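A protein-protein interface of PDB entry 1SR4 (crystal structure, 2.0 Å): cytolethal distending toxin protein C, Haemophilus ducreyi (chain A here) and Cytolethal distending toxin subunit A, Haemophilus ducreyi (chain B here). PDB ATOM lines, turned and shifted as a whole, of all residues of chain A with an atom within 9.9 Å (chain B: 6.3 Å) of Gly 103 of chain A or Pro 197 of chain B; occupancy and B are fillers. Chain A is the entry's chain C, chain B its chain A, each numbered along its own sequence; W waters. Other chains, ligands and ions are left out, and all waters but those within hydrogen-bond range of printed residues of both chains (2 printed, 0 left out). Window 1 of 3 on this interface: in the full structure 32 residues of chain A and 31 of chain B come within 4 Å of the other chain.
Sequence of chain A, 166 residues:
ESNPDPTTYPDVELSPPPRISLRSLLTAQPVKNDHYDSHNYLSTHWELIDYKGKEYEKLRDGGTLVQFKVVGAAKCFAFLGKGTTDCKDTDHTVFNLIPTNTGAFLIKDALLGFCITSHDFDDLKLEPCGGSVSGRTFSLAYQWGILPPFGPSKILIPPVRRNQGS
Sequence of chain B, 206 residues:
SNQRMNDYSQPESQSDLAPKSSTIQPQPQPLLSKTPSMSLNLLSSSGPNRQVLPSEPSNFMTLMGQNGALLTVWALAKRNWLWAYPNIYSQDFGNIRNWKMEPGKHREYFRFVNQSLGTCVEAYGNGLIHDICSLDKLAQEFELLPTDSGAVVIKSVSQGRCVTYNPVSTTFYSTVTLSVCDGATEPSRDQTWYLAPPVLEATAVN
Among the printed residues, pairs that only touch across the chains: Thr 102 of chain A with Pro 198 of chain B (3.5 Å), Leu 25 of chain A with Pro 197 of chain B (3.7 Å), Ala 104 of chain A with Pro 197 of chain B (3.7 Å), Gly 103 of chain A with Pro 197 of chain B (3.8 Å), Thr 102 of chain A with Pro 197 of chain B (3.8 Å), Leu 140 of chain A with Leu 200 of chain B (3.9 Å), Leu 147 of chain A with Leu 195 of chain B (3.9 Å), Arg 23 of chain A with Met 64 of chain B (3.9 Å), Leu 147 of chain A with Met 64 of chain B (3.9 Å), Leu 147 of chain A with Ala 196 of chain B (3.98 Å) and Leu 140 of chain A with Val 199 of chain B (3.98 Å).
Of the printed residues of chain B, Leu 25 of chain A touches Pro 197.
Of the printed residues of chain B, Thr 102 of chain A touches Pro 197 and Pro 198.
Printed residues of chain B within 4 Å of Ala 104 of chain A: Pro 197.
Of the printed residues of chain B, Leu 140 of chain A touches Val 199 (3.98 Å) and Leu 200 (3.9 Å).
No residue of chain A comes within 4 Å of Thr 62 of chain B.
Ala 196 of chain B touches just one residue of chain A: Leu 147 (3.98 Å).
Of chain A, only Leu 25 (3.7 Å), Thr 102 (3.8 Å), Gly 103 (3.8 Å) and Ala 104 (3.7 Å) come within 4 Å of Pro 197 of chain B.
Of chain A, only Thr 102 comes within 4 Å of Pro 198 of chain B.
Printed residues of chain A within 4 Å of Leu 200 of chain B: Leu 140 and Gln 143.
The nearest printed residue of chain B that does not touch Thr 102 of chain A is Leu 200 of chain B (4.7 Å).
O of Ala 196 of chain B sits at hydrogen-bond distance from N of Thr 62 of chain B.
The backbone NH (N) of Val 199 of chain B is in hydrogen-bond range of the side-chain amide oxygen (OD1) of Asn 98 of chain B, 2.8 Å away.
The backbone carbonyl oxygen (O) of Ala 28 of chain A lies within hydrogen-bond range of the guanidinium group (NH1) of Arg 23 of chain A (2.8 Å).
O of Arg 23 of chain A lies within hydrogen-bond range of N of Gly 145 of chain A (2.8 Å).
N of Leu 25 of chain A sits at hydrogen-bond distance from O of Gln 143 of chain A (3.0 Å).
N of Ala 104 of chain A lies within hydrogen-bond range of OG1 of Thr 102 of chain A (3.2 Å).
Printed residues of chain B that touch a printed residue of chain A: Met 64, Leu 195, Ala 196, Pro 197, Pro 198, Val 199 and Leu 200.
Hydrophobic or aromatic side chains of chain B within 4 Å of the printed part of chain A: Met 64, Ala 196, Pro 197, Pro 198 and Val 199.
Water W2 lies within hydrogen-bond range of the side-chain amide oxygen (OE1) of Gln 143 of chain A (2.7 Å), the side-chain hydroxyl (OG1) of Thr 102 of chain A (2.7 Å) and the backbone carbonyl oxygen (O) of Pro 198 of chain B (2.7 Å).
Water W1 bridges the backbone carbonyl oxygen (O) of Thr 102 of chain A and the backbone carbonyl oxygen (O) of Phe 60 of chain B.
The side-chain amide nitrogen of Gln 143 of chain A lies within hydrogen-bond range of the backbone carbonyl oxygen of Leu 200 of chain B.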
ATOM      1  N   SER A  21      16.301 -24.556   9.668  1.00  0.00           N
ATOM      2  CA  SER A  21      16.280 -25.828  10.361  1.00  0.00           C
ATOM      3  C   SER A  21      17.293 -25.501  11.467  1.00  0.00           C
ATOM      4  O   SER A  21      18.274 -24.798  11.223  1.00  0.00           O
ATOM      5  CB  SER A  21      16.754 -27.006   9.509  1.00  0.00           C
ATOM      6  OG  SER A  21      15.648 -27.631   8.860  1.00  0.00           O
ATOM      7  N   LEU A  22      17.021 -25.965  12.679  1.00  0.00           N
ATOM      8  CA  LEU A  22      17.886 -25.714  13.823  1.00  0.00           C
ATOM      9  C   LEU A  22      18.592 -27.019  14.144  1.00  0.00           C
ATOM     10  O   LEU A  22      17.938 -27.997  14.490  1.00  0.00           O
ATOM     11  CB  LEU A  22      17.023 -25.266  15.005  1.00  0.00           C
ATOM     12  CG  LEU A  22      17.688 -24.850  16.320  1.00  0.00           C
ATOM     13  CD1 LEU A  22      18.669 -23.703  16.091  1.00  0.00           C
ATOM     14  CD2 LEU A  22      16.588 -24.415  17.296  1.00  0.00           C
ATOM     15  N   ARG A  23      19.920 -27.028  14.035  1.00  0.00           N
ATOM     16  CA  ARG A  23      20.695 -28.234  14.277  1.00  0.00           C
ATOM     17  C   ARG A  23      21.768 -28.097  15.357  1.00  0.00           C
ATOM     18  O   ARG A  23      22.459 -27.091  15.438  1.00  0.00           O
ATOM     19  CB  ARG A  23      21.411 -28.686  12.989  1.00  0.00           C
ATOM     20  CG  ARG A  23      20.521 -29.087  11.822  1.00  0.00           C
ATOM     21  CD  ARG A  23      21.378 -29.426  10.614  1.00  0.00           C
ATOM     22  NE  ARG A  23      20.603 -29.739   9.419  1.00  0.00           N
ATOM     23  CZ  ARG A  23      20.366 -30.972   8.969  1.00  0.00           C
ATOM     24  NH1 ARG A  23      20.848 -32.030   9.617  1.00  0.00           N
ATOM     25  NH2 ARG A  23      19.649 -31.148   7.859  1.00  0.00           N
ATOM     26  N   SER A  24      21.913 -29.131  16.167  1.00  0.00           N
ATOM     27  CA  SER A  24      22.967 -29.148  17.178  1.00  0.00           C
ATOM     28  C   SER A  24      24.248 -29.356  16.378  1.00  0.00           C
ATOM     29  O   SER A  24      24.277 -30.205  15.486  1.00  0.00           O
ATOM     30  CB  SER A  24      22.789 -30.348  18.111  1.00  0.00           C
ATOM     31  OG  SER A  24      24.014 -30.649  18.765  1.00  0.00           O
ATOM     32  N   LEU A  25      25.303 -28.613  16.677  1.00  0.00           N
ATOM     33  CA  LEU A  25      26.533 -28.819  15.928  1.00  0.00           C
ATOM     34  C   LEU A  25      27.248 -30.075  16.389  1.00  0.00           C
ATOM     35  O   LEU A  25      28.182 -30.544  15.739  1.00  0.00           O
ATOM     36  CB  LEU A  25      27.464 -27.616  16.045  1.00  0.00           C
ATOM     37  CG  LEU A  25      26.906 -26.359  15.379  1.00  0.00           C
ATOM     38  CD1 LEU A  25      28.053 -25.362  15.198  1.00  0.00           C
ATOM     39  CD2 LEU A  25      26.287 -26.709  14.016  1.00  0.00           C
ATOM     40  N   LEU A  26      26.795 -30.638  17.503  1.00  0.00           N
ATOM     41  CA  LEU A  26      27.407 -31.858  17.993  1.00  0.00           C
ATOM     42  C   LEU A  26      26.742 -33.073  17.338  1.00  0.00           C
ATOM     43  O   LEU A  26      27.426 -33.950  16.842  1.00  0.00           O
ATOM     44  CB  LEU A  26      27.284 -31.942  19.522  1.00  0.00           C
ATOM     45  CG  LEU A  26      27.991 -33.127  20.199  1.00  0.00           C
ATOM     46  CD1 LEU A  26      28.279 -32.789  21.681  1.00  0.00           C
ATOM     47  CD2 LEU A  26      27.103 -34.382  20.098  1.00  0.00           C
ATOM     48  N   ALA A  28      24.256 -32.790  14.847  1.00  0.00           N
ATOM     49  CA  ALA A  28      23.853 -32.435  13.478  1.00  0.00           C
ATOM     50  C   ALA A  28      22.379 -32.763  13.221  1.00  0.00           C
ATOM     51  O   ALA A  28      21.897 -32.631  12.097  1.00  0.00           O
ATOM     52  CB  ALA A  28      24.719 -33.155  12.441  1.00  0.00           C
ATOM     53  N   LEU A  97      19.217 -15.787  21.197  1.00  0.00           N
ATOM     54  CA  LEU A  97      20.377 -16.093  20.354  1.00  0.00           C
ATOM     55  C   LEU A  97      21.611 -15.303  20.776  1.00  0.00           C
ATOM     56  O   LEU A  97      21.598 -14.082  20.807  1.00  0.00           O
ATOM     57  CB  LEU A  97      20.077 -15.792  18.873  1.00  0.00           C
ATOM     58  CG  LEU A  97      18.822 -16.419  18.235  1.00  0.00           C
ATOM     59  CD1 LEU A  97      18.780 -16.127  16.724  1.00  0.00           C
ATOM     60  CD2 LEU A  97      18.824 -17.933  18.473  1.00  0.00           C
ATOM     61  N   ILE A  98      22.678 -16.030  21.074  1.00  0.00           N
ATOM     62  CA  ILE A  98      23.964 -15.469  21.501  1.00  0.00           C
ATOM     63  C   ILE A  98      24.969 -15.751  20.367  1.00  0.00           C
ATOM     64  O   ILE A  98      25.293 -16.905  20.106  1.00  0.00           O
ATOM     65  CB  ILE A  98      24.489 -16.191  22.788  1.00  0.00           C
ATOM     66  CG1 ILE A  98      23.506 -16.013  23.957  1.00  0.00           C
ATOM     67  CG2 ILE A  98      25.904 -15.706  23.134  1.00  0.00           C
ATOM     68  CD1 ILE A  98      23.142 -14.553  24.298  1.00  0.00           C
ATOM     69  N   PRO A  99      25.465 -14.709  19.687  1.00  0.00           N
ATOM     70  CA  PRO A  99      26.429 -14.922  18.601  1.00  0.00           C
ATOM     71  C   PRO A  99      27.801 -15.328  19.145  1.00  0.00           C
ATOM     72  O   PRO A  99      28.119 -15.076  20.310  1.00  0.00           O
ATOM     73  CB  PRO A  99      26.466 -13.564  17.885  1.00  0.00           C
ATOM     74  CG  PRO A  99      26.259 -12.586  19.009  1.00  0.00           C
ATOM     75  CD  PRO A  99      25.186 -13.271  19.889  1.00  0.00           C
ATOM     76  N   THR A 100      28.609 -15.951  18.288  1.00  0.00           N
ATOM     77  CA  THR A 100      29.952 -16.406  18.660  1.00  0.00           C
ATOM     78  C   THR A 100      30.953 -16.042  17.565  1.00  0.00           C
ATOM     79  O   THR A 100      30.562 -15.569  16.488  1.00  0.00           O
ATOM     80  CB  THR A 100      30.014 -17.937  18.814  1.00  0.00           C
ATOM     81  OG1 THR A 100      29.888 -18.547  17.527  1.00  0.00           O
ATOM     82  CG2 THR A 100      28.914 -18.437  19.720  1.00  0.00           C
ATOM     83  N   ASN A 101      32.238 -16.284  17.827  1.00  0.00           N
ATOM     84  CA  ASN A 101      33.265 -15.984  16.835  1.00  0.00           C
ATOM     85  C   ASN A 101      33.306 -17.000  15.699  1.00  0.00           C
ATOM     86  O   ASN A 101      34.133 -16.865  14.784  1.00  0.00           O
ATOM     87  CB  ASN A 101      34.665 -15.878  17.486  1.00  0.00           C
ATOM     88  CG  ASN A 101      35.124 -17.169  18.184  1.00  0.00           C
ATOM     89  OD1 ASN A 101      34.337 -18.087  18.443  1.00  0.00           O
ATOM     90  ND2 ASN A 101      36.422 -17.230  18.504  1.00  0.00           N
ATOM     91  N   THR A 102      32.447 -18.018  15.738  1.00  0.00           N
ATOM     92  CA  THR A 102      32.455 -18.998  14.646  1.00  0.00           C
ATOM     93  C   THR A 102      31.217 -18.970  13.756  1.00  0.00           C
ATOM     94  O   THR A 102      31.220 -19.582  12.680  1.00  0.00           O
ATOM     95  CB  THR A 102      32.577 -20.456  15.135  1.00  0.00           C
ATOM     96  OG1 THR A 102      31.346 -20.863  15.737  1.00  0.00           O
ATOM     97  CG2 THR A 102      33.725 -20.606  16.139  1.00  0.00           C
ATOM     98  N   GLY A 103      30.163 -18.278  14.187  1.00  0.00           N
ATOM     99  CA  GLY A 103      28.942 -18.265  13.392  1.00  0.00           C
ATOM    100  C   GLY A 103      27.924 -19.228  13.994  1.00  0.00           C
ATOM    101  O   GLY A 103      26.767 -19.271  13.583  1.00  0.00           O
ATOM    102  N   ALA A 104      28.377 -20.049  14.937  1.00  0.00           N
ATOM    103  CA  ALA A 104      27.475 -20.943  15.641  1.00  0.00           C
ATOM    104  C   ALA A 104      26.804 -20.034  16.673  1.00  0.00           C
ATOM    105  O   ALA A 104      27.301 -18.932  16.948  1.00  0.00           O
ATOM    106  CB  ALA A 104      28.257 -22.021  16.359  1.00  0.00           C
ATOM    107  N   PHE A 105      25.702 -20.504  17.249  1.00  0.00           N
ATOM    108  CA  PHE A 105      24.995 -19.748  18.270  1.00  0.00           C
ATOM    109  C   PHE A 105      24.812 -20.579  19.516  1.00  0.00           C
ATOM    110  O   PHE A 105      24.734 -21.819  19.453  1.00  0.00           O
ATOM    111  CB  PHE A 105      23.591 -19.338  17.791  1.00  0.00           C
ATOM    112  CG  PHE A 105      23.612 -18.326  16.699  1.00  0.00           C
ATOM    113  CD1 PHE A 105      23.674 -16.964  17.003  1.00  0.00           C
ATOM    114  CD2 PHE A 105      23.679 -18.729  15.370  1.00  0.00           C
ATOM    115  CE1 PHE A 105      23.812 -16.008  15.988  1.00  0.00           C
ATOM    116  CE2 PHE A 105      23.816 -17.772  14.348  1.00  0.00           C
ATOM    117  CZ  PHE A 105      23.884 -16.418  14.666  1.00  0.00           C
ATOM    118  N   LEU A 106      24.773 -19.877  20.643  1.00  0.00           N
ATOM    119  CA  LEU A 106      24.452 -20.495  21.916  1.00  0.00           C
ATOM    120  C   LEU A 106      22.986 -20.070  21.989  1.00  0.00           C
ATOM    121  O   LEU A 106      22.614 -19.035  21.426  1.00  0.00           O
ATOM    122  CB  LEU A 106      25.218 -19.852  23.076  1.00  0.00           C
ATOM    123  CG  LEU A 106      26.432 -20.601  23.616  1.00  0.00           C
ATOM    124  CD1 LEU A 106      27.517 -20.566  22.569  1.00  0.00           C
ATOM    125  CD2 LEU A 106      26.923 -19.959  24.928  1.00  0.00           C
ATOM    126  N   ILE A 107      22.139 -20.848  22.643  1.00  0.00           N
ATOM    127  CA  ILE A 107      20.742 -20.451  22.753  1.00  0.00           C
ATOM    128  C   ILE A 107      20.286 -20.564  24.197  1.00  0.00           C
ATOM    129  O   ILE A 107      20.390 -21.638  24.798  1.00  0.00           O
ATOM    130  CB  ILE A 107      19.806 -21.328  21.891  1.00  0.00           C
ATOM    131  CG1 ILE A 107      20.231 -21.268  20.419  1.00  0.00           C
ATOM    132  CG2 ILE A 107      18.358 -20.827  22.041  1.00  0.00           C
ATOM    133  CD1 ILE A 107      19.390 -22.150  19.490  1.00  0.00           C
ATOM    134  N   LEU A 140      30.952 -28.001  21.389  1.00  0.00           N
ATOM    135  CA  LEU A 140      29.853 -28.149  20.431  1.00  0.00           C
ATOM    136  C   LEU A 140      28.515 -28.509  21.074  1.00  0.00           C
ATOM    137  O   LEU A 140      27.461 -28.259  20.499  1.00  0.00           O
ATOM    138  CB  LEU A 140      30.213 -29.211  19.379  1.00  0.00           C
ATOM    139  CG  LEU A 140      31.431 -28.887  18.501  1.00  0.00           C
ATOM    140  CD1 LEU A 140      31.899 -30.140  17.744  1.00  0.00           C
ATOM    141  CD2 LEU A 140      31.045 -27.786  17.504  1.00  0.00           C
ATOM    142  N   GLN A 143      26.530 -25.525  21.132  1.00  0.00           N
ATOM    143  CA  GLN A 143      26.429 -24.830  19.858  1.00  0.00           C
ATOM    144  C   GLN A 143      25.341 -25.286  18.920  1.00  0.00           C
ATOM    145  O   GLN A 143      25.106 -26.475  18.757  1.00  0.00           O
ATOM    146  CB  GLN A 143      27.767 -24.928  19.139  1.00  0.00           C
ATOM    147  CG  GLN A 143      28.964 -24.401  19.945  1.00  0.00           C
ATOM    148  CD  GLN A 143      30.233 -24.495  19.133  1.00  0.00           C
ATOM    149  OE1 GLN A 143      30.213 -24.277  17.919  1.00  0.00           O
ATOM    150  NE2 GLN A 143      31.349 -24.801  19.790  1.00  0.00           N
ATOM    151  N   TRP A 144      24.724 -24.310  18.266  1.00  0.00           N
ATOM    152  CA  TRP A 144      23.634 -24.544  17.339  1.00  0.00           C
ATOM    153  C   TRP A 144      23.839 -23.874  15.987  1.00  0.00           C
ATOM    154  O   TRP A 144      24.373 -22.765  15.901  1.00  0.00           O
ATOM    155  CB  TRP A 144      22.347 -24.022  17.976  1.00  0.00           C
ATOM    156  CG  TRP A 144      22.062 -24.773  19.234  1.00  0.00           C
ATOM    157  CD1 TRP A 144      22.547 -24.513  20.485  1.00  0.00           C
ATOM    158  CD2 TRP A 144      21.367 -26.015  19.321  1.00  0.00           C
ATOM    159  NE1 TRP A 144      22.204 -25.535  21.346  1.00  0.00           N
ATOM    160  CE2 TRP A 144      21.481 -26.470  20.656  1.00  0.00           C
ATOM    161  CE3 TRP A 144      20.665 -26.796  18.393  1.00  0.00           C
ATOM    162  CZ2 TRP A 144      20.915 -27.679  21.089  1.00  0.00           C
ATOM    163  CZ3 TRP A 144      20.106 -27.998  18.819  1.00  0.00           C
ATOM    164  CH2 TRP A 144      20.235 -28.426  20.155  1.00  0.00           C
ATOM    165  N   GLY A 145      23.402 -24.545  14.931  1.00  0.00           N
ATOM    166  CA  GLY A 145      23.505 -23.953  13.610  1.00  0.00           C
ATOM    167  C   GLY A 145      22.115 -23.527  13.172  1.00  0.00           C
ATOM    168  O   GLY A 145      21.173 -24.312  13.273  1.00  0.00           O
ATOM    169  N   ILE A 146      21.965 -22.274  12.749  1.00  0.00           N
ATOM    170  CA  ILE A 146      20.681 -21.772  12.250  1.00  0.00           C
ATOM    171  C   ILE A 146      20.947 -21.898  10.754  1.00  0.00           C
ATOM    172  O   ILE A 146      21.576 -21.034  10.151  1.00  0.00           O
ATOM    173  CB  ILE A 146      20.451 -20.289  12.648  1.00  0.00           C
ATOM    174  CG1 ILE A 146      20.141 -20.172  14.149  1.00  0.00           C
ATOM    175  CG2 ILE A 146      19.210 -19.730  11.930  1.00  0.00           C
ATOM    176  CD1 ILE A 146      21.172 -20.779  15.038  1.00  0.00           C
ATOM    177  N   LEU A 147      20.466 -22.988  10.175  1.00  0.00           N
ATOM    178  CA  LEU A 147      20.767 -23.324   8.785  1.00  0.00           C
ATOM    179  C   LEU A 147      19.600 -23.398   7.810  1.00  0.00           C
ATOM    180  O   LEU A 147      18.437 -23.307   8.204  1.00  0.00           O
ATOM    181  CB  LEU A 147      21.509 -24.676   8.786  1.00  0.00           C
ATOM    182  CG  LEU A 147      22.830 -24.700   9.583  1.00  0.00           C
ATOM    183  CD1 LEU A 147      23.251 -26.123   9.928  1.00  0.00           C
ATOM    184  CD2 LEU A 147      23.921 -24.020   8.764  1.00  0.00           C
ATOM    185  N   PRO A 148      19.906 -23.562   6.505  1.00  0.00           N
ATOM    186  CA  PRO A 148      18.830 -23.655   5.512  1.00  0.00           C
ATOM    187  C   PRO A 148      17.909 -24.813   5.938  1.00  0.00           C
ATOM    188  O   PRO A 148      18.354 -25.783   6.558  1.00  0.00           O
ATOM    189  CB  PRO A 148      19.584 -23.942   4.207  1.00  0.00           C
ATOM    190  CG  PRO A 148      20.921 -23.221   4.416  1.00  0.00           C
ATOM    191  CD  PRO A 148      21.238 -23.593   5.858  1.00  0.00           C
ATOM    192  N   PHE B  60      37.179 -20.111   9.384  1.00  0.00           N
ATOM    193  CA  PHE B  60      36.873 -21.457   8.939  1.00  0.00           C
ATOM    194  C   PHE B  60      35.405 -21.813   8.989  1.00  0.00           C
ATOM    195  O   PHE B  60      34.612 -21.152   9.635  1.00  0.00           O
ATOM    196  CB  PHE B  60      37.699 -22.442   9.766  1.00  0.00           C
ATOM    197  CG  PHE B  60      39.160 -22.191   9.657  1.00  0.00           C
ATOM    198  CD1 PHE B  60      39.883 -22.694   8.579  1.00  0.00           C
ATOM    199  CD2 PHE B  60      39.798 -21.361  10.565  1.00  0.00           C
ATOM    200  CE1 PHE B  60      41.220 -22.364   8.413  1.00  0.00           C
ATOM    201  CE2 PHE B  60      41.150 -21.026  10.403  1.00  0.00           C
ATOM    202  CZ  PHE B  60      41.854 -21.527   9.329  1.00  0.00           C
ATOM    203  N   MET B  61      35.061 -22.884   8.297  1.00  0.00           N
ATOM    204  CA  MET B  61      33.686 -23.341   8.239  1.00  0.00           C
ATOM    205  C   MET B  61      33.669 -24.805   7.837  1.00  0.00           C
ATOM    206  O   MET B  61      34.729 -25.415   7.637  1.00  0.00           O
ATOM    207  CB  MET B  61      32.931 -22.501   7.204  1.00  0.00           C
ATOM    208  CG  MET B  61      33.664 -22.322   5.861  1.00  0.00           C
ATOM    209  SD  MET B  61      33.607 -23.749   4.746  1.00  0.00           S
ATOM    210  CE  MET B  61      31.972 -23.497   4.036  1.00  0.00           C
ATOM    211  N   THR B  62      32.473 -25.378   7.748  1.00  0.00           N
ATOM    212  CA  THR B  62      32.347 -26.741   7.258  1.00  0.00           C
ATOM    213  C   THR B  62      31.302 -26.749   6.143  1.00  0.00           C
ATOM    214  O   THR B  62      30.462 -25.846   6.046  1.00  0.00           O
ATOM    215  CB  THR B  62      31.862 -27.745   8.328  1.00  0.00           C
ATOM    216  OG1 THR B  62      30.645 -27.262   8.910  1.00  0.00           O
ATOM    217  CG2 THR B  62      32.923 -27.964   9.411  1.00  0.00           C
ATOM    218  N   MET B  64      28.386 -28.883   5.109  1.00  0.00           N
ATOM    219  CA  MET B  64      27.550 -29.908   5.726  1.00  0.00           C
ATOM    220  C   MET B  64      26.451 -30.414   4.808  1.00  0.00           C
ATOM    221  O   MET B  64      25.711 -29.621   4.230  1.00  0.00           O
ATOM    222  CB  MET B  64      26.912 -29.332   7.008  1.00  0.00           C
ATOM    223  CG  MET B  64      25.978 -30.314   7.733  1.00  0.00           C
ATOM    224  SD  MET B  64      24.973 -29.565   9.070  1.00  0.00           S
ATOM    225  CE  MET B  64      26.192 -29.102  10.310  1.00  0.00           C
ATOM    226  N   LEU B  70      29.918 -33.901   7.264  1.00  0.00           N
ATOM    227  CA  LEU B  70      30.806 -32.798   6.886  1.00  0.00           C
ATOM    228  C   LEU B  70      31.890 -33.247   5.887  1.00  0.00           C
ATOM    229  O   LEU B  70      32.525 -34.283   6.086  1.00  0.00           O
ATOM    230  CB  LEU B  70      31.474 -32.258   8.158  1.00  0.00           C
ATOM    231  CG  LEU B  70      30.555 -32.047   9.371  1.00  0.00           C
ATOM    232  CD1 LEU B  70      31.404 -31.858  10.652  1.00  0.00           C
ATOM    233  CD2 LEU B  70      29.657 -30.856   9.124  1.00  0.00           C
ATOM    234  N   ASN B  98      37.623 -28.922   8.962  1.00  0.00           N
ATOM    235  CA  ASN B  98      37.337 -27.509   8.726  1.00  0.00           C
ATOM    236  C   ASN B  98      38.097 -26.948   7.543  1.00  0.00           C
ATOM    237  O   ASN B  98      39.239 -27.313   7.303  1.00  0.00           O
ATOM    238  CB  ASN B  98      37.675 -26.665   9.974  1.00  0.00           C
ATOM    239  CG  ASN B  98      36.882 -27.088  11.186  1.00  0.00           C
ATOM    240  OD1 ASN B  98      35.674 -27.303  11.098  1.00  0.00           O
ATOM    241  ND2 ASN B  98      37.554 -27.211  12.330  1.00  0.00           N
ATOM    242  N   LEU B 195      26.471 -24.051   4.148  1.00  0.00           N
ATOM    243  CA  LEU B 195      27.696 -23.354   4.521  1.00  0.00           C
ATOM    244  C   LEU B 195      27.480 -23.234   6.028  1.00  0.00           C
ATOM    245  O   LEU B 195      26.644 -22.450   6.478  1.00  0.00           O
ATOM    246  CB  LEU B 195      27.732 -21.987   3.814  1.00  0.00           C
ATOM    247  CG  LEU B 195      27.747 -22.182   2.277  1.00  0.00           C
ATOM    248  CD1 LEU B 195      27.548 -20.883   1.531  1.00  0.00           C
ATOM    249  CD2 LEU B 195      29.061 -22.827   1.895  1.00  0.00           C
ATOM    250  N   ALA B 196      28.236 -24.013   6.800  1.00  0.00           N
ATOM    251  CA  ALA B 196      28.036 -24.091   8.249  1.00  0.00           C
ATOM    252  C   ALA B 196      29.216 -23.694   9.127  1.00  0.00           C
ATOM    253  O   ALA B 196      30.346 -23.560   8.648  1.00  0.00           O
ATOM    254  CB  ALA B 196      27.585 -25.565   8.607  1.00  0.00           C
ATOM    255  N   PRO B 197      28.971 -23.510  10.441  1.00  0.00           N
ATOM    256  CA  PRO B 197      30.064 -23.133  11.344  1.00  0.00           C
ATOM    257  C   PRO B 197      31.067 -24.279  11.395  1.00  0.00           C
ATOM    258  O   PRO B 197      30.708 -25.440  11.197  1.00  0.00           O
ATOM    259  CB  PRO B 197      29.367 -22.952  12.705  1.00  0.00           C
ATOM    260  CG  PRO B 197      27.914 -22.657  12.335  1.00  0.00           C
ATOM    261  CD  PRO B 197      27.697 -23.607  11.173  1.00  0.00           C
ATOM    262  N   PRO B 198      32.337 -23.966  11.663  1.00  0.00           N
ATOM    263  CA  PRO B 198      33.384 -24.985  11.740  1.00  0.00           C
ATOM    264  C   PRO B 198      33.173 -25.809  12.999  1.00  0.00           C
ATOM    265  O   PRO B 198      32.454 -25.370  13.906  1.00  0.00           O
ATOM    266  CB  PRO B 198      34.661 -24.152  11.829  1.00  0.00           C
ATOM    267  CG  PRO B 198      34.213 -22.975  12.699  1.00  0.00           C
ATOM    268  CD  PRO B 198      32.843 -22.637  12.073  1.00  0.00           C
ATOM    269  N   VAL B 199      33.762 -27.001  13.068  1.00  0.00           N
ATOM    270  CA  VAL B 199      33.645 -27.765  14.298  1.00  0.00           C
ATOM    271  C   VAL B 199      34.846 -27.340  15.142  1.00  0.00           C
ATOM    272  O   VAL B 199      35.947 -27.880  15.021  1.00  0.00           O
ATOM    273  CB  VAL B 199      33.616 -29.296  14.077  1.00  0.00           C
ATOM    274  CG1 VAL B 199      32.171 -29.734  13.794  1.00  0.00           C
ATOM    275  CG2 VAL B 199      34.507 -29.700  12.931  1.00  0.00           C
ATOM    276  N   LEU B 200      34.605 -26.331  15.979  1.00  0.00           N
ATOM    277  CA  LEU B 200      35.622 -25.749  16.858  1.00  0.00           C
ATOM    278  C   LEU B 200      34.948 -25.240  18.127  1.00  0.00           C
ATOM    279  O   LEU B 200      33.730 -25.067  18.146  1.00  0.00           O
ATOM    280  CB  LEU B 200      36.294 -24.552  16.164  1.00  0.00           C
ATOM    281  CG  LEU B 200      37.129 -24.747  14.887  1.00  0.00           C
ATOM    282  CD1 LEU B 200      37.505 -23.397  14.291  1.00  0.00           C
ATOM    283  CD2 LEU B 200      38.386 -25.539  15.221  1.00  0.00           C
HETATM  284  O   HOH W   1      33.401 -19.031  11.238  1.00  0.00           O
HETATM  285  O   HOH W   2      31.499 -23.549  15.704  1.00  0.00           O
